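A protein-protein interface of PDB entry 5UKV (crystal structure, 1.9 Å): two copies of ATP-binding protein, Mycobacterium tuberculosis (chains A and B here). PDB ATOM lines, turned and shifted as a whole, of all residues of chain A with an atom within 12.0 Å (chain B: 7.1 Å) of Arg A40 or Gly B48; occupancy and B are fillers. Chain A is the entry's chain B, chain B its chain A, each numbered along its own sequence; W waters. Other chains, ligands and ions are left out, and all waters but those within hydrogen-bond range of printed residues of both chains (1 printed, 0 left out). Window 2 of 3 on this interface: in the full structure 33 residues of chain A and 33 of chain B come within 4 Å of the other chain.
Ile A54 touches Leu B51, but with the chains exchanged Leu A51 does not touch Ile B54 (4.3 Å).
Ala A36 touches Glu B55. Arg A40 touches Leu B51. CD1 of Ile A54 touches CD1 of Leu B51, 3.9 Å away.
Hydrophobic or aromatic side chains of chain B within 4 Å of the printed part of chain A: Leu B51. Along chain B the printed residues that touch a printed residue of chain A span positions 48 to 55. Of the 22 printed residues of chain A, 3 touch a printed residue of chain B. Printed residues of chain A that touch a printed residue of chain B: Ala A36, Arg A40 and Ile A54. Hydrophobic or aromatic side chains of chain A within 4 Å of the printed part of chain B: Ala A36 and Ile A54. Among the printed residues, 6 pairs touch across the chains.
Water W1 lies within hydrogen-bond range of NH2 of Arg A40 (2.6 Å) and O of Gly B48 (3.1 Å).
The backbone NH (N) of Gly B48 sits at hydrogen-bond distance from the side-chain carboxylate (OD1) of Asp B46 (2.9 Å).
The guanidinium group (NH1) of Arg A40 lies within hydrogen-bond range of the backbone carbonyl oxygen (O) of Gly B48. N of Ser B52 lies close to NH1 of Arg A40. The guanidinium group (NE) of Arg A40 is in salt-bridge range of the side-chain carboxylate (OE1) of Glu B55, 2.8 Å away.
Gly A34 touches none of the printed residues of chain B. Of the printed residues of chain B, Ala A36 touches Glu B55. Arg A40 touches just these residues of chain B: Gly B48, Leu B51, Ser B52 and Glu B55. Gly A42 touches none of the printed residues of chain B. Printed residues of chain B within 4 Å of Ile A54: Leu B51. Of chain A, only Arg A40 (3.0 Å) comes within 4 Å of Gly B48. Leu B51 touches two residues of chain A. Ser B52 touches just one residue of chain A: Arg A40 (3.2 Å). The nearest printed residue of chain B that does not touch Ile A54 is Ile B54 (4.2 Å).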
ATOM      1  N   THR A  31      -9.821  19.174  18.346  1.00  0.00           N
ATOM      2  CA  THR A  31     -11.179  19.697  18.371  1.00  0.00           C
ATOM      3  C   THR A  31     -11.307  21.027  17.653  1.00  0.00           C
ATOM      4  O   THR A  31     -12.215  21.227  16.832  1.00  0.00           O
ATOM      5  CB  THR A  31     -11.663  19.907  19.865  1.00  0.00           C
ATOM      6  OG1 THR A  31     -11.766  18.661  20.507  1.00  0.00           O
ATOM      7  CG2 THR A  31     -13.015  20.459  19.965  1.00  0.00           C
ATOM      8  N   ILE A  32     -10.422  21.955  17.968  1.00  0.00           N
ATOM      9  CA  ILE A  32     -10.489  23.284  17.318  1.00  0.00           C
ATOM     10  C   ILE A  32     -10.359  23.090  15.778  1.00  0.00           C
ATOM     11  O   ILE A  32     -11.101  23.733  14.999  1.00  0.00           O
ATOM     12  CB  ILE A  32      -9.428  24.255  17.901  1.00  0.00           C
ATOM     13  CG1 ILE A  32      -9.825  24.620  19.319  1.00  0.00           C
ATOM     14  CG2 ILE A  32      -9.152  25.454  16.982  1.00  0.00           C
ATOM     15  CD1 ILE A  32      -8.667  25.218  20.048  1.00  0.00           C
ATOM     16  N   ARG A  33      -9.353  22.304  15.380  1.00  0.00           N
ATOM     17  CA  ARG A  33      -9.074  22.052  13.969  1.00  0.00           C
ATOM     18  C   ARG A  33     -10.183  21.412  13.213  1.00  0.00           C
ATOM     19  O   ARG A  33     -10.552  21.844  12.074  1.00  0.00           O
ATOM     20  CB  ARG A  33      -7.892  21.104  13.851  1.00  0.00           C
ATOM     21  CG  ARG A  33      -7.685  20.481  12.410  1.00  0.00           C
ATOM     22  CD  ARG A  33      -6.354  19.707  12.270  1.00  0.00           C
ATOM     23  NE  ARG A  33      -6.487  18.243  12.174  1.00  0.00           N
ATOM     24  CZ  ARG A  33      -5.453  17.414  12.293  1.00  0.00           C
ATOM     25  NH1 ARG A  33      -4.230  17.881  12.518  1.00  0.00           N
ATOM     26  NH2 ARG A  33      -5.640  16.104  12.176  1.00  0.00           N
ATOM     27  N   GLY A  34     -10.723  20.355  13.815  1.00  0.00           N
ATOM     28  CA  GLY A  34     -11.843  19.683  13.225  1.00  0.00           C
ATOM     29  C   GLY A  34     -13.118  20.448  13.074  1.00  0.00           C
ATOM     30  O   GLY A  34     -13.767  20.426  12.000  1.00  0.00           O
ATOM     31  N   PHE A  35     -13.457  21.221  14.132  1.00  0.00           N
ATOM     32  CA  PHE A  35     -14.650  22.044  14.094  1.00  0.00           C
ATOM     33  C   PHE A  35     -14.409  23.146  13.089  1.00  0.00           C
ATOM     34  O   PHE A  35     -15.307  23.466  12.305  1.00  0.00           O
ATOM     35  CB  PHE A  35     -15.039  22.652  15.493  1.00  0.00           C
ATOM     36  CG  PHE A  35     -15.750  21.715  16.474  1.00  0.00           C
ATOM     37  CD1 PHE A  35     -15.383  20.454  16.690  1.00  0.00           C
ATOM     38  CD2 PHE A  35     -16.876  22.209  17.249  1.00  0.00           C
ATOM     39  CE1 PHE A  35     -16.130  19.606  17.546  1.00  0.00           C
ATOM     40  CE2 PHE A  35     -17.597  21.388  18.121  1.00  0.00           C
ATOM     41  CZ  PHE A  35     -17.202  20.047  18.278  1.00  0.00           C
ATOM     42  N   ALA A  36     -13.232  23.816  13.125  1.00  0.00           N
ATOM     43  CA  ALA A  36     -13.015  24.877  12.178  1.00  0.00           C
ATOM     44  C   ALA A  36     -13.195  24.422  10.720  1.00  0.00           C
ATOM     45  O   ALA A  36     -13.844  25.089   9.896  1.00  0.00           O
ATOM     46  CB  ALA A  36     -11.610  25.467  12.363  1.00  0.00           C
ATOM     47  N   GLU A  37     -12.625  23.302  10.416  1.00  0.00           N
ATOM     48  CA  GLU A  37     -12.880  22.682   9.093  1.00  0.00           C
ATOM     49  C   GLU A  37     -14.319  22.445   8.682  1.00  0.00           C
ATOM     50  O   GLU A  37     -14.726  22.787   7.526  1.00  0.00           O
ATOM     51  CB  GLU A  37     -12.080  21.382   8.872  1.00  0.00           C
ATOM     52  CG  GLU A  37     -11.991  21.116   7.345  1.00  0.00           C
ATOM     53  CD  GLU A  37     -12.261  19.721   6.865  1.00  0.00           C
ATOM     54  OE1 GLU A  37     -12.798  18.832   7.598  1.00  0.00           O
ATOM     55  OE2 GLU A  37     -11.949  19.527   5.649  1.00  0.00           O
ATOM     56  N   LEU A  38     -15.111  21.874   9.569  1.00  0.00           N
ATOM     57  CA  LEU A  38     -16.510  21.588   9.305  1.00  0.00           C
ATOM     58  C   LEU A  38     -17.235  22.884   8.987  1.00  0.00           C
ATOM     59  O   LEU A  38     -18.035  22.975   8.056  1.00  0.00           O
ATOM     60  CB  LEU A  38     -17.100  20.937  10.524  1.00  0.00           C
ATOM     61  CG  LEU A  38     -18.239  20.028  10.521  1.00  0.00           C
ATOM     62  CD1 LEU A  38     -17.925  18.723   9.756  1.00  0.00           C
ATOM     63  CD2 LEU A  38     -18.630  19.708  11.979  1.00  0.00           C
ATOM     64  N   TYR A  39     -16.978  23.903   9.811  1.00  0.00           N
ATOM     65  CA  TYR A  39     -17.591  25.231   9.627  1.00  0.00           C
ATOM     66  C   TYR A  39     -17.214  25.930   8.326  1.00  0.00           C
ATOM     67  O   TYR A  39     -18.092  26.495   7.589  1.00  0.00           O
ATOM     68  CB  TYR A  39     -17.408  26.127  10.873  1.00  0.00           C
ATOM     69  CG  TYR A  39     -18.429  25.895  11.993  1.00  0.00           C
ATOM     70  CD1 TYR A  39     -18.255  24.891  12.900  1.00  0.00           C
ATOM     71  CD2 TYR A  39     -19.585  26.626  12.072  1.00  0.00           C
ATOM     72  CE1 TYR A  39     -19.185  24.670  13.875  1.00  0.00           C
ATOM     73  CE2 TYR A  39     -20.551  26.437  13.074  1.00  0.00           C
ATOM     74  CZ  TYR A  39     -20.366  25.391  13.965  1.00  0.00           C
ATOM     75  OH  TYR A  39     -21.270  25.204  14.979  1.00  0.00           O
ATOM     76  N   ARG A  40     -15.964  25.860   7.991  1.00  0.00           N
ATOM     77  CA  ARG A  40     -15.491  26.438   6.752  1.00  0.00           C
ATOM     78  C   ARG A  40     -16.133  25.774   5.541  1.00  0.00           C
ATOM     79  O   ARG A  40     -16.304  26.383   4.581  1.00  0.00           O
ATOM     80  CB  ARG A  40     -13.990  26.380   6.642  1.00  0.00           C
ATOM     81  CG  ARG A  40     -13.301  27.371   7.542  1.00  0.00           C
ATOM     82  CD  ARG A  40     -11.954  27.788   7.013  1.00  0.00           C
ATOM     83  NE  ARG A  40     -11.220  28.670   7.885  1.00  0.00           N
ATOM     84  CZ  ARG A  40     -11.207  29.977   7.761  1.00  0.00           C
ATOM     85  NH1 ARG A  40     -10.496  30.690   8.586  1.00  0.00           N
ATOM     86  NH2 ARG A  40     -11.891  30.572   6.813  1.00  0.00           N
ATOM     87  N   GLN A  41     -16.385  24.494   5.622  1.00  0.00           N
ATOM     88  CA  GLN A  41     -16.967  23.668   4.573  1.00  0.00           C
ATOM     89  C   GLN A  41     -18.457  23.849   4.409  1.00  0.00           C
ATOM     90  O   GLN A  41     -19.053  23.296   3.446  1.00  0.00           O
ATOM     91  CB  GLN A  41     -16.562  22.184   4.746  1.00  0.00           C
ATOM     92  CG  GLN A  41     -15.089  21.990   4.473  1.00  0.00           C
ATOM     93  CD  GLN A  41     -14.770  22.296   3.025  1.00  0.00           C
ATOM     94  OE1 GLN A  41     -15.625  22.177   2.135  1.00  0.00           O
ATOM     95  NE2 GLN A  41     -13.569  22.698   2.775  1.00  0.00           N
ATOM     96  N   GLY A  42     -19.092  24.576   5.343  1.00  0.00           N
ATOM     97  CA  GLY A  42     -20.532  24.804   5.288  1.00  0.00           C
ATOM     98  C   GLY A  42     -21.401  23.711   5.773  1.00  0.00           C
ATOM     99  O   GLY A  42     -22.622  23.763   5.522  1.00  0.00           O
ATOM    100  N   ALA A  43     -20.827  22.805   6.606  1.00  0.00           N
ATOM    101  CA  ALA A  43     -21.499  21.666   7.039  1.00  0.00           C
ATOM    102  C   ALA A  43     -22.129  21.928   8.381  1.00  0.00           C
ATOM    103  O   ALA A  43     -22.869  21.051   8.892  1.00  0.00           O
ATOM    104  CB  ALA A  43     -20.479  20.506   7.226  1.00  0.00           C
ATOM    105  N   ALA A  44     -21.877  23.096   8.976  1.00  0.00           N
ATOM    106  CA  ALA A  44     -22.476  23.445  10.294  1.00  0.00           C
ATOM    107  C   ALA A  44     -23.135  24.846  10.443  1.00  0.00           C
ATOM    108  O   ALA A  44     -22.891  25.803   9.717  1.00  0.00           O
ATOM    109  CB  ALA A  44     -21.430  23.214  11.365  1.00  0.00           C
ATOM    110  N   ARG A  45     -23.927  24.985  11.478  1.00  0.00           N
ATOM    111  CA  ARG A  45     -24.566  26.239  11.759  1.00  0.00           C
ATOM    112  C   ARG A  45     -24.259  26.765  13.178  1.00  0.00           C
ATOM    113  O   ARG A  45     -23.929  26.044  14.058  1.00  0.00           O
ATOM    114  CB  ARG A  45     -26.068  26.156  11.528  1.00  0.00           C
ATOM    115  CG  ARG A  45     -26.789  25.130  12.373  1.00  0.00           C
ATOM    116  CD  ARG A  45     -28.319  25.122  12.267  1.00  0.00           C
ATOM    117  NE  ARG A  45     -28.871  24.833  10.967  1.00  0.00           N
ATOM    118  CZ  ARG A  45     -29.121  23.630  10.513  1.00  0.00           C
ATOM    119  NH1 ARG A  45     -29.620  23.480   9.327  1.00  0.00           N
ATOM    120  NH2 ARG A  45     -28.877  22.578  11.244  1.00  0.00           N
ATOM    121  N   ASP A  46     -24.356  28.061  13.329  1.00  0.00           N
ATOM    122  CA  ASP A  46     -24.108  28.785  14.648  1.00  0.00           C
ATOM    123  C   ASP A  46     -22.678  28.893  14.905  1.00  0.00           C
ATOM    124  O   ASP A  46     -22.020  28.182  15.635  1.00  0.00           O
ATOM    125  CB  ASP A  46     -24.828  28.086  15.800  1.00  0.00           C
ATOM    126  CG  ASP A  46     -24.948  28.962  17.005  1.00  0.00           C
ATOM    127  OD1 ASP A  46     -24.222  29.954  17.020  1.00  0.00           O
ATOM    128  OD2 ASP A  46     -25.704  28.528  17.908  1.00  0.00           O
ATOM    129  N   VAL A  47     -22.156  29.895  14.270  1.00  0.00           N
ATOM    130  CA  VAL A  47     -20.780  30.253  14.387  1.00  0.00           C
ATOM    131  C   VAL A  47     -20.447  30.695  15.818  1.00  0.00           C
ATOM    132  O   VAL A  47     -19.348  30.490  16.284  1.00  0.00           O
ATOM    133  CB  VAL A  47     -20.508  31.356  13.345  1.00  0.00           C
ATOM    134  CG1 VAL A  47     -19.072  31.826  13.411  1.00  0.00           C
ATOM    135  CG2 VAL A  47     -20.776  30.769  11.959  1.00  0.00           C
ATOM    136  N   GLY A  48     -21.425  31.215  16.525  1.00  0.00           N
ATOM    137  CA  GLY A  48     -21.210  31.524  17.935  1.00  0.00           C
ATOM    138  C   GLY A  48     -20.924  30.291  18.749  1.00  0.00           C
ATOM    139  O   GLY A  48     -20.142  30.376  19.615  1.00  0.00           O
ATOM    140  N   MET A  49     -21.524  29.132  18.448  1.00  0.00           N
ATOM    141  CA  MET A  49     -21.114  27.901  19.094  1.00  0.00           C
ATOM    142  C   MET A  49     -19.703  27.410  18.740  1.00  0.00           C
ATOM    143  O   MET A  49     -19.025  26.770  19.565  1.00  0.00           O
ATOM    144  CB  MET A  49     -22.161  26.885  18.724  1.00  0.00           C
ATOM    145  CG  MET A  49     -22.316  25.755  19.748  1.00  0.00           C
ATOM    146  SD  MET A  49     -23.609  24.454  18.925  1.00  0.00           S
ATOM    147  CE  MET A  49     -25.307  25.175  19.520  1.00  0.00           C
ATOM    148  N   LEU A  50     -19.252  27.592  17.486  1.00  0.00           N
ATOM    149  CA  LEU A  50     -17.903  27.280  17.168  1.00  0.00           C
ATOM    150  C   LEU A  50     -16.978  28.138  18.040  1.00  0.00           C
ATOM    151  O   LEU A  50     -16.050  27.633  18.631  1.00  0.00           O
ATOM    152  CB  LEU A  50     -17.609  27.651  15.692  1.00  0.00           C
ATOM    153  CG  LEU A  50     -16.177  27.676  15.296  1.00  0.00           C
ATOM    154  CD1 LEU A  50     -15.546  26.300  15.299  1.00  0.00           C
ATOM    155  CD2 LEU A  50     -16.057  28.255  13.947  1.00  0.00           C
ATOM    156  N   LEU A  51     -17.180  29.447  18.005  1.00  0.00           N
ATOM    157  CA  LEU A  51     -16.300  30.358  18.790  1.00  0.00           C
ATOM    158  C   LEU A  51     -16.373  30.124  20.286  1.00  0.00           C
ATOM    159  O   LEU A  51     -15.356  30.309  20.978  1.00  0.00           O
ATOM    160  CB  LEU A  51     -16.625  31.824  18.547  1.00  0.00           C
ATOM    161  CG  LEU A  51     -15.851  32.477  17.394  1.00  0.00           C
ATOM    162  CD1 LEU A  51     -14.357  32.589  17.771  1.00  0.00           C
ATOM    163  CD2 LEU A  51     -15.891  31.748  16.087  1.00  0.00           C
ATOM    164  N   ILE A  54     -14.236  27.067  20.915  1.00  0.00           N
ATOM    165  CA  ILE A  54     -12.815  27.467  20.839  1.00  0.00           C
ATOM    166  C   ILE A  54     -12.427  28.159  22.198  1.00  0.00           C
ATOM    167  O   ILE A  54     -11.351  27.829  22.791  1.00  0.00           O
ATOM    168  CB  ILE A  54     -12.582  28.377  19.646  1.00  0.00           C
ATOM    169  CG1 ILE A  54     -12.615  27.581  18.360  1.00  0.00           C
ATOM    170  CG2 ILE A  54     -11.222  28.984  19.722  1.00  0.00           C
ATOM    171  CD1 ILE A  54     -12.782  28.388  17.059  1.00  0.00           C
ATOM    172  N   ARG B  45     -15.762  41.691  12.620  1.00  0.00           N
ATOM    173  CA  ARG B  45     -16.481  41.946  11.337  1.00  0.00           C
ATOM    174  C   ARG B  45     -16.141  40.707  10.440  1.00  0.00           C
ATOM    175  O   ARG B  45     -17.014  39.994   9.999  1.00  0.00           O
ATOM    176  CB  ARG B  45     -16.052  43.243  10.570  1.00  0.00           C
ATOM    177  CG  ARG B  45     -15.821  44.560  11.286  1.00  0.00           C
ATOM    178  CD  ARG B  45     -15.265  45.726  10.414  1.00  0.00           C
ATOM    179  NE  ARG B  45     -15.973  46.893  10.848  1.00  0.00           N
ATOM    180  CZ  ARG B  45     -17.130  47.263  10.332  1.00  0.00           C
ATOM    181  NH1 ARG B  45     -17.780  48.274  10.869  1.00  0.00           N
ATOM    182  NH2 ARG B  45     -17.645  46.629   9.260  1.00  0.00           N
ATOM    183  N   ASP B  46     -14.866  40.407  10.215  1.00  0.00           N
ATOM    184  CA  ASP B  46     -14.445  39.279   9.373  1.00  0.00           C
ATOM    185  C   ASP B  46     -14.004  38.103  10.231  1.00  0.00           C
ATOM    186  O   ASP B  46     -12.833  37.904  10.455  1.00  0.00           O
ATOM    187  CB  ASP B  46     -13.392  39.685   8.390  1.00  0.00           C
ATOM    188  CG  ASP B  46     -12.925  38.545   7.484  1.00  0.00           C
ATOM    189  OD1 ASP B  46     -13.380  37.405   7.618  1.00  0.00           O
ATOM    190  OD2 ASP B  46     -11.918  38.778   6.758  1.00  0.00           O
ATOM    191  N   VAL B  47     -14.953  37.265  10.580  1.00  0.00           N
ATOM    192  CA  VAL B  47     -14.696  36.094  11.353  1.00  0.00           C
ATOM    193  C   VAL B  47     -13.785  35.128  10.629  1.00  0.00           C
ATOM    194  O   VAL B  47     -13.133  34.347  11.252  1.00  0.00           O
ATOM    195  CB  VAL B  47     -15.965  35.392  11.796  1.00  0.00           C
ATOM    196  CG1 VAL B  47     -15.635  34.417  12.877  1.00  0.00           C
ATOM    197  CG2 VAL B  47     -16.908  36.379  12.388  1.00  0.00           C
ATOM    198  N   GLY B  48     -13.821  35.114   9.314  1.00  0.00           N
ATOM    199  CA  GLY B  48     -12.909  34.231   8.569  1.00  0.00           C
ATOM    200  C   GLY B  48     -11.437  34.493   8.801  1.00  0.00           C
ATOM    201  O   GLY B  48     -10.621  33.617   8.987  1.00  0.00           O
ATOM    202  N   MET B  49     -11.112  35.771   8.872  1.00  0.00           N
ATOM    203  CA  MET B  49      -9.783  36.199   9.226  1.00  0.00           C
ATOM    204  C   MET B  49      -9.441  35.867  10.662  1.00  0.00           C
ATOM    205  O   MET B  49      -8.369  35.388  10.884  1.00  0.00           O
ATOM    206  CB  MET B  49      -9.537  37.676   8.981  1.00  0.00           C
ATOM    207  CG  MET B  49      -8.052  37.859   9.151  1.00  0.00           C
ATOM    208  SD  MET B  49      -7.523  39.691   8.761  1.00  0.00           S
ATOM    209  CE  MET B  49      -7.530  39.362   6.831  1.00  0.00           C
ATOM    210  N   LEU B  50     -10.363  36.081  11.589  1.00  0.00           N
ATOM    211  CA  LEU B  50     -10.201  35.803  12.970  1.00  0.00           C
ATOM    212  C   LEU B  50      -9.927  34.322  13.136  1.00  0.00           C
ATOM    213  O   LEU B  50      -9.030  33.931  13.770  1.00  0.00           O
ATOM    214  CB  LEU B  50     -11.512  36.152  13.647  1.00  0.00           C
ATOM    215  CG  LEU B  50     -11.587  36.312  15.133  1.00  0.00           C
ATOM    216  CD1 LEU B  50     -10.859  37.526  15.593  1.00  0.00           C
ATOM    217  CD2 LEU B  50     -12.954  36.275  15.761  1.00  0.00           C
ATOM    218  N   LEU B  51     -10.712  33.520  12.474  1.00  0.00           N
ATOM    219  CA  LEU B  51     -10.612  32.038  12.496  1.00  0.00           C
ATOM    220  C   LEU B  51      -9.317  31.488  11.894  1.00  0.00           C
ATOM    221  O   LEU B  51      -8.687  30.539  12.472  1.00  0.00           O
ATOM    222  CB  LEU B  51     -11.833  31.383  11.792  1.00  0.00           C
ATOM    223  CG  LEU B  51     -11.896  29.843  11.908  1.00  0.00           C
ATOM    224  CD1 LEU B  51     -11.934  29.426  13.399  1.00  0.00           C
ATOM    225  CD2 LEU B  51     -13.083  29.373  11.234  1.00  0.00           C
ATOM    226  N   SER B  52      -8.864  32.151  10.853  1.00  0.00           N
ATOM    227  CA  SER B  52      -7.632  31.818  10.220  1.00  0.00           C
ATOM    228  C   SER B  52      -6.443  31.983  11.181  1.00  0.00           C
ATOM    229  O   SER B  52      -5.624  31.148  11.303  1.00  0.00           O
ATOM    230  CB  SER B  52      -7.465  32.791   9.079  1.00  0.00           C
ATOM    231  OG  SER B  52      -6.566  32.334   8.175  1.00  0.00           O
ATOM    232  N   ARG B  53      -6.422  33.082  11.909  1.00  0.00           N
ATOM    233  CA  ARG B  53      -5.368  33.301  12.862  1.00  0.00           C
ATOM    234  C   ARG B  53      -5.456  32.258  13.957  1.00  0.00           C
ATOM    235  O   ARG B  53      -4.472  31.761  14.377  1.00  0.00           O
ATOM    236  CB  ARG B  53      -5.398  34.693  13.452  1.00  0.00           C
ATOM    237  CG  ARG B  53      -4.384  34.903  14.575  1.00  0.00           C
ATOM    238  CD  ARG B  53      -2.945  34.558  14.176  1.00  0.00           C
ATOM    239  NE  ARG B  53      -2.524  35.278  12.996  1.00  0.00           N
ATOM    240  CZ  ARG B  53      -1.345  35.184  12.418  1.00  0.00           C
ATOM    241  NH1 ARG B  53      -0.428  34.385  12.904  1.00  0.00           N
ATOM    242  NH2 ARG B  53      -1.078  35.921  11.357  1.00  0.00           N
ATOM    243  N   ILE B  54      -6.658  31.980  14.415  1.00  0.00           N
ATOM    244  CA  ILE B  54      -6.858  30.990  15.411  1.00  0.00           C
ATOM    245  C   ILE B  54      -6.361  29.641  14.968  1.00  0.00           C
ATOM    246  O   ILE B  54      -5.651  28.972  15.707  1.00  0.00           O
ATOM    247  CB  ILE B  54      -8.309  30.906  15.908  1.00  0.00           C
ATOM    248  CG1 ILE B  54      -8.632  32.129  16.766  1.00  0.00           C
ATOM    249  CG2 ILE B  54      -8.522  29.537  16.606  1.00  0.00           C
ATOM    250  CD1 ILE B  54     -10.140  32.344  17.032  1.00  0.00           C
ATOM    251  N   GLU B  55      -6.652  29.251  13.744  1.00  0.00           N
ATOM    252  CA  GLU B  55      -6.207  27.999  13.194  1.00  0.00           C
ATOM    253  C   GLU B  55      -4.690  27.925  13.092  1.00  0.00           C
ATOM    254  O   GLU B  55      -4.102  26.946  13.375  1.00  0.00           O
ATOM    255  CB  GLU B  55      -6.830  27.777  11.823  1.00  0.00           C
ATOM    256  CG  GLU B  55      -8.279  27.391  11.876  1.00  0.00           C
ATOM    257  CD  GLU B  55      -8.935  27.217  10.499  1.00  0.00           C
ATOM    258  OE1 GLU B  55      -9.415  28.187   9.932  1.00  0.00           O
ATOM    259  OE2 GLU B  55      -8.974  26.095   9.999  1.00  0.00           O
HETATM  260  O   HOH W   1     -10.921  32.868   6.041  1.00  0.00           O
